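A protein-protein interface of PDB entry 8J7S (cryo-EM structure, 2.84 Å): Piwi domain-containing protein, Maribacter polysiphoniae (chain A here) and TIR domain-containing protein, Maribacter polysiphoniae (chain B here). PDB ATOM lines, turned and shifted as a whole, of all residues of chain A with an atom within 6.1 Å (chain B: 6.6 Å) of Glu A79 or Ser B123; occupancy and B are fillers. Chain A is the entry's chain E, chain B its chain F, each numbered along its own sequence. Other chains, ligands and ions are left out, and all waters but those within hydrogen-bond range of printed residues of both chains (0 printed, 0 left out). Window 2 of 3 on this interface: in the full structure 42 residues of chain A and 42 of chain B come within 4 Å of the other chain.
OE1 of Gln A61 lies close to OE2 of Glu A79 (2.9 Å).
N of Lys B121 sits at hydrogen-bond distance from OD1 of Asp B119 (2.8 Å).
OG of Ser B123 lies within hydrogen-bond range of N of Arg B126, 3.0 Å away.
The side-chain amino group (NZ) of Lys B129 is in hydrogen-bond range of the backbone carbonyl oxygen (O) of Ala B125.
Gln A61 touches Met B122 (O to O, 3.9 Å).
Lys B121 touches Lys A62.
Met B122 touches Lys A62.
CG of Pro A63 touches NE1 of Trp B124, 3.2 Å away.
Pro A76 touches Trp B124.
Glu A79 touches Ser B123 (OE1 to CB, 3.5 Å).
Glu A79 touches Ala B125 (OE1 to CB, 3.7 Å).
N of Ala A80 touches CB of Ala B125, at 3.9 Å.
Of chain B, only Ser B123 (3.5 Å) and Ala B125 (3.7 Å) come within 4 Å of Glu A79.
Of the printed residues of chain A, Ser B123 touches Glu A79.
Printed residues of chain B within 4 Å of Pro A63: Trp B124.
Printed residues of chain A within 4 Å of Lys B121: Lys A62 (3.9 Å).
Printed residues of chain A within 4 Å of Ala B125: Glu A79 (3.7 Å) and Ala A80 (3.9 Å).
Of the printed residues of chain A, Trp B124 touches Pro A63 (3.2 Å) and Pro A76 (3.99 Å).
The nearest residue of chain B that does not touch Glu A79 is Arg B126 (4.3 Å).
The nearest printed residue of chain B that does not touch Gln A61 is Ser B123 (4.2 Å).
Of the 14 printed residues of chain A, 6 touch a printed residue of chain B.
Hydrophobic or aromatic side chains of chain A within 4 Å of the printed part of chain B: Pro A63 and Pro A76.
Of the 11 printed residues of chain B, 5 touch a printed residue of chain A.
Hydrophobic or aromatic side chains of chain B within 4 Å of the printed part of chain A: Trp B124 and Ala B125.
Among the printed residues, no Asp or Glu carboxylate lies within 4 Å of a Lys or Arg side-chain nitrogen of the other chain.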
ATOM      1  N   ILE A  60      -8.242  19.200 -17.820  1.00  0.00           N
ATOM      2  CA  ILE A  60      -7.518  19.671 -19.000  1.00  0.00           C
ATOM      3  C   ILE A  60      -8.452  19.959 -20.170  1.00  0.00           C
ATOM      4  O   ILE A  60      -7.999  20.243 -21.284  1.00  0.00           O
ATOM      5  CB  ILE A  60      -6.397  18.692 -19.404  1.00  0.00           C
ATOM      6  CG1 ILE A  60      -6.905  17.605 -20.360  1.00  0.00           C
ATOM      7  CG2 ILE A  60      -5.701  18.141 -18.177  1.00  0.00           C
ATOM      8  CD1 ILE A  60      -5.823  16.661 -20.831  1.00  0.00           C
ATOM      9  N   GLN A  61      -9.761  19.927 -19.928  1.00  0.00           N
ATOM     10  CA  GLN A  61     -10.671  20.491 -20.917  1.00  0.00           C
ATOM     11  C   GLN A  61     -10.656  22.013 -20.877  1.00  0.00           C
ATOM     12  O   GLN A  61     -10.852  22.663 -21.912  1.00  0.00           O
ATOM     13  CB  GLN A  61     -12.094  19.969 -20.700  1.00  0.00           C
ATOM     14  CG  GLN A  61     -12.232  18.455 -20.725  1.00  0.00           C
ATOM     15  CD  GLN A  61     -11.892  17.846 -22.072  1.00  0.00           C
ATOM     16  OE1 GLN A  61     -12.352  18.312 -23.111  1.00  0.00           O
ATOM     17  NE2 GLN A  61     -11.083  16.793 -22.056  1.00  0.00           N
ATOM     18  N   LYS A  62     -10.421  22.591 -19.703  1.00  0.00           N
ATOM     19  CA  LYS A  62     -10.332  24.019 -19.446  1.00  0.00           C
ATOM     20  C   LYS A  62      -8.913  24.519 -19.684  1.00  0.00           C
ATOM     21  O   LYS A  62      -7.954  23.741 -19.649  1.00  0.00           O
ATOM     22  CB  LYS A  62     -10.766  24.309 -18.010  1.00  0.00           C
ATOM     23  CG  LYS A  62     -12.178  23.851 -17.697  1.00  0.00           C
ATOM     24  CD  LYS A  62     -12.518  24.055 -16.232  1.00  0.00           C
ATOM     25  CE  LYS A  62     -11.813  23.031 -15.360  1.00  0.00           C
ATOM     26  NZ  LYS A  62     -12.252  23.104 -13.941  1.00  0.00           N
ATOM     27  N   PRO A  63      -8.738  25.817 -19.939  1.00  0.00           N
ATOM     28  CA  PRO A  63      -7.390  26.341 -20.190  1.00  0.00           C
ATOM     29  C   PRO A  63      -6.505  26.265 -18.957  1.00  0.00           C
ATOM     30  O   PRO A  63      -6.964  26.393 -17.819  1.00  0.00           O
ATOM     31  CB  PRO A  63      -7.641  27.798 -20.597  1.00  0.00           C
ATOM     32  CG  PRO A  63      -9.100  27.900 -20.849  1.00  0.00           C
ATOM     33  CD  PRO A  63      -9.754  26.877 -20.005  1.00  0.00           C
ATOM     34  N   PRO A  76      -4.482  26.112 -24.168  1.00  0.00           N
ATOM     35  CA  PRO A  76      -5.866  26.581 -24.332  1.00  0.00           C
ATOM     36  C   PRO A  76      -6.912  25.563 -23.916  1.00  0.00           C
ATOM     37  O   PRO A  76      -7.984  25.957 -23.440  1.00  0.00           O
ATOM     38  CB  PRO A  76      -5.962  26.897 -25.833  1.00  0.00           C
ATOM     39  CG  PRO A  76      -4.585  26.699 -26.398  1.00  0.00           C
ATOM     40  CD  PRO A  76      -3.825  25.841 -25.453  1.00  0.00           C
ATOM     41  N   GLY A  77      -6.639  24.274 -24.079  1.00  0.00           N
ATOM     42  CA  GLY A  77      -7.621  23.228 -23.849  1.00  0.00           C
ATOM     43  C   GLY A  77      -7.558  22.241 -24.997  1.00  0.00           C
ATOM     44  O   GLY A  77      -7.286  22.603 -26.143  1.00  0.00           O
ATOM     45  N   PHE A  78      -7.829  20.971 -24.685  1.00  0.00           N
ATOM     46  CA  PHE A  78      -7.553  19.897 -25.637  1.00  0.00           C
ATOM     47  C   PHE A  78      -8.366  20.054 -26.917  1.00  0.00           C
ATOM     48  O   PHE A  78      -7.834  19.884 -28.021  1.00  0.00           O
ATOM     49  CB  PHE A  78      -7.828  18.537 -24.993  1.00  0.00           C
ATOM     50  CG  PHE A  78      -7.373  17.371 -25.825  1.00  0.00           C
ATOM     51  CD1 PHE A  78      -8.167  16.867 -26.842  1.00  0.00           C
ATOM     52  CD2 PHE A  78      -6.143  16.785 -25.596  1.00  0.00           C
ATOM     53  CE1 PHE A  78      -7.739  15.804 -27.610  1.00  0.00           C
ATOM     54  CE2 PHE A  78      -5.714  15.722 -26.359  1.00  0.00           C
ATOM     55  CZ  PHE A  78      -6.513  15.230 -27.367  1.00  0.00           C
ATOM     56  N   GLU A  79      -9.655  20.367 -26.792  1.00  0.00           N
ATOM     57  CA  GLU A  79     -10.494  20.496 -27.979  1.00  0.00           C
ATOM     58  C   GLU A  79     -10.068  21.686 -28.828  1.00  0.00           C
ATOM     59  O   GLU A  79     -10.120  21.626 -30.061  1.00  0.00           O
ATOM     60  CB  GLU A  79     -11.964  20.624 -27.580  1.00  0.00           C
ATOM     61  CG  GLU A  79     -12.276  20.224 -26.147  1.00  0.00           C
ATOM     62  CD  GLU A  79     -11.889  21.289 -25.137  1.00  0.00           C
ATOM     63  OE1 GLU A  79     -11.963  22.489 -25.473  1.00  0.00           O
ATOM     64  OE2 GLU A  79     -11.510  20.923 -24.008  1.00  0.00           O
ATOM     65  N   ALA A  80      -9.659  22.781 -28.184  1.00  0.00           N
ATOM     66  CA  ALA A  80      -9.193  23.947 -28.925  1.00  0.00           C
ATOM     67  C   ALA A  80      -7.935  23.622 -29.719  1.00  0.00           C
ATOM     68  O   ALA A  80      -7.826  23.964 -30.902  1.00  0.00           O
ATOM     69  CB  ALA A  80      -8.941  25.109 -27.965  1.00  0.00           C
ATOM     70  N   VAL A  81      -6.975  22.951 -29.083  1.00  0.00           N
ATOM     71  CA  VAL A  81      -5.710  22.645 -29.744  1.00  0.00           C
ATOM     72  C   VAL A  81      -5.914  21.635 -30.866  1.00  0.00           C
ATOM     73  O   VAL A  81      -5.438  21.829 -31.991  1.00  0.00           O
ATOM     74  CB  VAL A  81      -4.680  22.135 -28.720  1.00  0.00           C
ATOM     75  CG1 VAL A  81      -3.359  21.845 -29.401  1.00  0.00           C
ATOM     76  CG2 VAL A  81      -4.490  23.138 -27.614  1.00  0.00           C
ATOM     77  N   PHE A  82      -6.629  20.546 -30.584  1.00  0.00           N
ATOM     78  CA  PHE A  82      -6.561  19.349 -31.410  1.00  0.00           C
ATOM     79  C   PHE A  82      -7.843  19.037 -32.168  1.00  0.00           C
ATOM     80  O   PHE A  82      -7.851  18.091 -32.960  1.00  0.00           O
ATOM     81  CB  PHE A  82      -6.175  18.152 -30.538  1.00  0.00           C
ATOM     82  CG  PHE A  82      -4.721  18.118 -30.179  1.00  0.00           C
ATOM     83  CD1 PHE A  82      -3.753  18.123 -31.165  1.00  0.00           C
ATOM     84  CD2 PHE A  82      -4.323  18.107 -28.856  1.00  0.00           C
ATOM     85  CE1 PHE A  82      -2.418  18.096 -30.839  1.00  0.00           C
ATOM     86  CE2 PHE A  82      -2.991  18.083 -28.525  1.00  0.00           C
ATOM     87  CZ  PHE A  82      -2.037  18.075 -29.519  1.00  0.00           C
ATOM     88  N   ASP A  83      -8.905  19.821 -31.970  1.00  0.00           N
ATOM     89  CA  ASP A  83     -10.242  19.568 -32.524  1.00  0.00           C
ATOM     90  C   ASP A  83     -10.598  18.082 -32.495  1.00  0.00           C
ATOM     91  O   ASP A  83     -11.041  17.493 -33.482  1.00  0.00           O
ATOM     92  CB  ASP A  83     -10.400  20.154 -33.934  1.00  0.00           C
ATOM     93  CG  ASP A  83      -9.270  19.782 -34.869  1.00  0.00           C
ATOM     94  OD1 ASP A  83      -8.180  20.378 -34.756  1.00  0.00           O
ATOM     95  OD2 ASP A  83      -9.474  18.901 -35.730  1.00  0.00           O
ATOM     96  N   CYS A  84     -10.397  17.477 -31.327  1.00  0.00           N
ATOM     97  CA  CYS A  84     -10.815  16.115 -31.035  1.00  0.00           C
ATOM     98  C   CYS A  84     -11.639  16.137 -29.758  1.00  0.00           C
ATOM     99  O   CYS A  84     -11.919  17.198 -29.195  1.00  0.00           O
ATOM    100  CB  CYS A  84      -9.613  15.174 -30.878  1.00  0.00           C
ATOM    101  SG  CYS A  84      -8.583  14.982 -32.344  1.00  0.00           S
ATOM    102  N   LYS A  85     -12.031  14.956 -29.293  1.00  0.00           N
ATOM    103  CA  LYS A  85     -12.627  14.798 -27.974  1.00  0.00           C
ATOM    104  C   LYS A  85     -11.865  13.720 -27.222  1.00  0.00           C
ATOM    105  O   LYS A  85     -11.782  12.577 -27.683  1.00  0.00           O
ATOM    106  CB  LYS A  85     -14.115  14.450 -28.062  1.00  0.00           C
ATOM    107  CG  LYS A  85     -14.993  15.599 -28.528  1.00  0.00           C
ATOM    108  CD  LYS A  85     -16.186  15.111 -29.330  1.00  0.00           C
ATOM    109  CE  LYS A  85     -15.810  14.806 -30.765  1.00  0.00           C
ATOM    110  NZ  LYS A  85     -14.773  15.735 -31.283  1.00  0.00           N
ATOM    111  N   ASP B 119     -20.490  31.605 -23.165  1.00  0.00           N
ATOM    112  CA  ASP B 119     -19.720  31.098 -22.037  1.00  0.00           C
ATOM    113  C   ASP B 119     -18.441  30.422 -22.513  1.00  0.00           C
ATOM    114  O   ASP B 119     -18.471  29.578 -23.413  1.00  0.00           O
ATOM    115  CB  ASP B 119     -20.555  30.118 -21.215  1.00  0.00           C
ATOM    116  CG  ASP B 119     -20.033  29.955 -19.805  1.00  0.00           C
ATOM    117  OD1 ASP B 119     -18.921  30.448 -19.526  1.00  0.00           O
ATOM    118  OD2 ASP B 119     -20.728  29.331 -18.977  1.00  0.00           O
ATOM    119  N   PHE B 120     -17.318  30.800 -21.901  1.00  0.00           N
ATOM    120  CA  PHE B 120     -16.035  30.148 -22.125  1.00  0.00           C
ATOM    121  C   PHE B 120     -15.463  29.554 -20.845  1.00  0.00           C
ATOM    122  O   PHE B 120     -14.316  29.094 -20.850  1.00  0.00           O
ATOM    123  CB  PHE B 120     -15.018  31.125 -22.719  1.00  0.00           C
ATOM    124  CG  PHE B 120     -15.315  31.543 -24.129  1.00  0.00           C
ATOM    125  CD1 PHE B 120     -16.237  32.538 -24.394  1.00  0.00           C
ATOM    126  CD2 PHE B 120     -14.642  30.967 -25.189  1.00  0.00           C
ATOM    127  CE1 PHE B 120     -16.497  32.929 -25.688  1.00  0.00           C
ATOM    128  CE2 PHE B 120     -14.896  31.358 -26.482  1.00  0.00           C
ATOM    129  CZ  PHE B 120     -15.827  32.339 -26.732  1.00  0.00           C
ATOM    130  N   LYS B 121     -16.221  29.565 -19.745  1.00  0.00           N
ATOM    131  CA  LYS B 121     -15.707  29.017 -18.493  1.00  0.00           C
ATOM    132  C   LYS B 121     -15.441  27.523 -18.611  1.00  0.00           C
ATOM    133  O   LYS B 121     -14.565  26.984 -17.926  1.00  0.00           O
ATOM    134  CB  LYS B 121     -16.687  29.288 -17.354  1.00  0.00           C
ATOM    135  CG  LYS B 121     -16.957  30.752 -17.087  1.00  0.00           C
ATOM    136  CD  LYS B 121     -18.276  30.920 -16.358  1.00  0.00           C
ATOM    137  CE  LYS B 121     -18.637  32.381 -16.192  1.00  0.00           C
ATOM    138  NZ  LYS B 121     -19.235  32.643 -14.855  1.00  0.00           N
ATOM    139  N   MET B 122     -16.192  26.835 -19.472  1.00  0.00           N
ATOM    140  CA  MET B 122     -16.030  25.393 -19.610  1.00  0.00           C
ATOM    141  C   MET B 122     -14.958  25.045 -20.635  1.00  0.00           C
ATOM    142  O   MET B 122     -14.011  24.314 -20.330  1.00  0.00           O
ATOM    143  CB  MET B 122     -17.366  24.753 -19.989  1.00  0.00           C
ATOM    144  CG  MET B 122     -18.262  24.288 -18.827  1.00  0.00           C
ATOM    145  SD  MET B 122     -17.504  23.447 -17.408  1.00  0.00           S
ATOM    146  CE  MET B 122     -16.863  24.794 -16.408  1.00  0.00           C
ATOM    147  N   SER B 123     -15.092  25.558 -21.854  1.00  0.00           N
ATOM    148  CA  SER B 123     -14.145  25.251 -22.913  1.00  0.00           C
ATOM    149  C   SER B 123     -14.150  26.387 -23.922  1.00  0.00           C
ATOM    150  O   SER B 123     -15.205  26.950 -24.222  1.00  0.00           O
ATOM    151  CB  SER B 123     -14.491  23.926 -23.597  1.00  0.00           C
ATOM    152  OG  SER B 123     -15.253  24.149 -24.769  1.00  0.00           O
ATOM    153  N   TRP B 124     -12.966  26.721 -24.438  1.00  0.00           N
ATOM    154  CA  TRP B 124     -12.865  27.767 -25.448  1.00  0.00           C
ATOM    155  C   TRP B 124     -13.352  27.302 -26.813  1.00  0.00           C
ATOM    156  O   TRP B 124     -13.784  28.129 -27.621  1.00  0.00           O
ATOM    157  CB  TRP B 124     -11.425  28.268 -25.557  1.00  0.00           C
ATOM    158  CG  TRP B 124     -10.958  29.070 -24.387  1.00  0.00           C
ATOM    159  CD1 TRP B 124     -11.646  29.328 -23.240  1.00  0.00           C
ATOM    160  CD2 TRP B 124      -9.691  29.720 -24.249  1.00  0.00           C
ATOM    161  NE1 TRP B 124     -10.887  30.101 -22.396  1.00  0.00           N
ATOM    162  CE2 TRP B 124      -9.681  30.355 -22.994  1.00  0.00           C
ATOM    163  CE3 TRP B 124      -8.562  29.827 -25.067  1.00  0.00           C
ATOM    164  CZ2 TRP B 124      -8.587  31.084 -22.536  1.00  0.00           C
ATOM    165  CZ3 TRP B 124      -7.481  30.552 -24.612  1.00  0.00           C
ATOM    166  CH2 TRP B 124      -7.499  31.169 -23.359  1.00  0.00           C
ATOM    167  N   ALA B 125     -13.288  26.000 -27.095  1.00  0.00           N
ATOM    168  CA  ALA B 125     -13.734  25.511 -28.396  1.00  0.00           C
ATOM    169  C   ALA B 125     -15.247  25.612 -28.539  1.00  0.00           C
ATOM    170  O   ALA B 125     -15.752  25.993 -29.603  1.00  0.00           O
ATOM    171  CB  ALA B 125     -13.271  24.070 -28.604  1.00  0.00           C
ATOM    172  N   ARG B 126     -15.988  25.280 -27.479  1.00  0.00           N
ATOM    173  CA  ARG B 126     -17.440  25.413 -27.524  1.00  0.00           C
ATOM    174  C   ARG B 126     -17.853  26.868 -27.693  1.00  0.00           C
ATOM    175  O   ARG B 126     -18.729  27.185 -28.508  1.00  0.00           O
ATOM    176  CB  ARG B 126     -18.060  24.823 -26.258  1.00  0.00           C
ATOM    177  CG  ARG B 126     -19.431  24.192 -26.456  1.00  0.00           C
ATOM    178  CD  ARG B 126     -19.383  22.962 -27.359  1.00  0.00           C
ATOM    179  NE  ARG B 126     -18.094  22.280 -27.329  1.00  0.00           N
ATOM    180  CZ  ARG B 126     -17.721  21.413 -26.397  1.00  0.00           C
ATOM    181  NH1 ARG B 126     -18.519  21.096 -25.389  1.00  0.00           N
ATOM    182  NH2 ARG B 126     -16.517  20.854 -26.475  1.00  0.00           N
ATOM    183  N   GLY B 127     -17.227  27.769 -26.936  1.00  0.00           N
ATOM    184  CA  GLY B 127     -17.524  29.180 -27.093  1.00  0.00           C
ATOM    185  C   GLY B 127     -17.166  29.696 -28.472  1.00  0.00           C
ATOM    186  O   GLY B 127     -17.870  30.538 -29.034  1.00  0.00           O
ATOM    187  N   LEU B 128     -16.066  29.198 -29.039  1.00  0.00           N
ATOM    188  CA  LEU B 128     -15.691  29.603 -30.388  1.00  0.00           C
ATOM    189  C   LEU B 128     -16.728  29.147 -31.406  1.00  0.00           C
ATOM    190  O   LEU B 128     -17.093  29.908 -32.307  1.00  0.00           O
ATOM    191  CB  LEU B 128     -14.308  29.052 -30.734  1.00  0.00           C
ATOM    192  CG  LEU B 128     -13.688  29.538 -32.044  1.00  0.00           C
ATOM    193  CD1 LEU B 128     -13.601  31.053 -32.067  1.00  0.00           C
ATOM    194  CD2 LEU B 128     -12.317  28.922 -32.233  1.00  0.00           C
ATOM    195  N   LYS B 129     -17.217  27.912 -31.277  1.00  0.00           N
ATOM    196  CA  LYS B 129     -18.267  27.448 -32.182  1.00  0.00           C
ATOM    197  C   LYS B 129     -19.533  28.277 -32.015  1.00  0.00           C
ATOM    198  O   LYS B 129     -20.226  28.574 -32.997  1.00  0.00           O
ATOM    199  CB  LYS B 129     -18.567  25.965 -31.953  1.00  0.00           C
ATOM    200  CG  LYS B 129     -17.370  25.031 -32.063  1.00  0.00           C
ATOM    201  CD  LYS B 129     -16.339  25.517 -33.073  1.00  0.00           C
ATOM    202  CE  LYS B 129     -14.958  24.976 -32.741  1.00  0.00           C
ATOM    203  NZ  LYS B 129     -14.277  25.794 -31.702  1.00  0.00           N
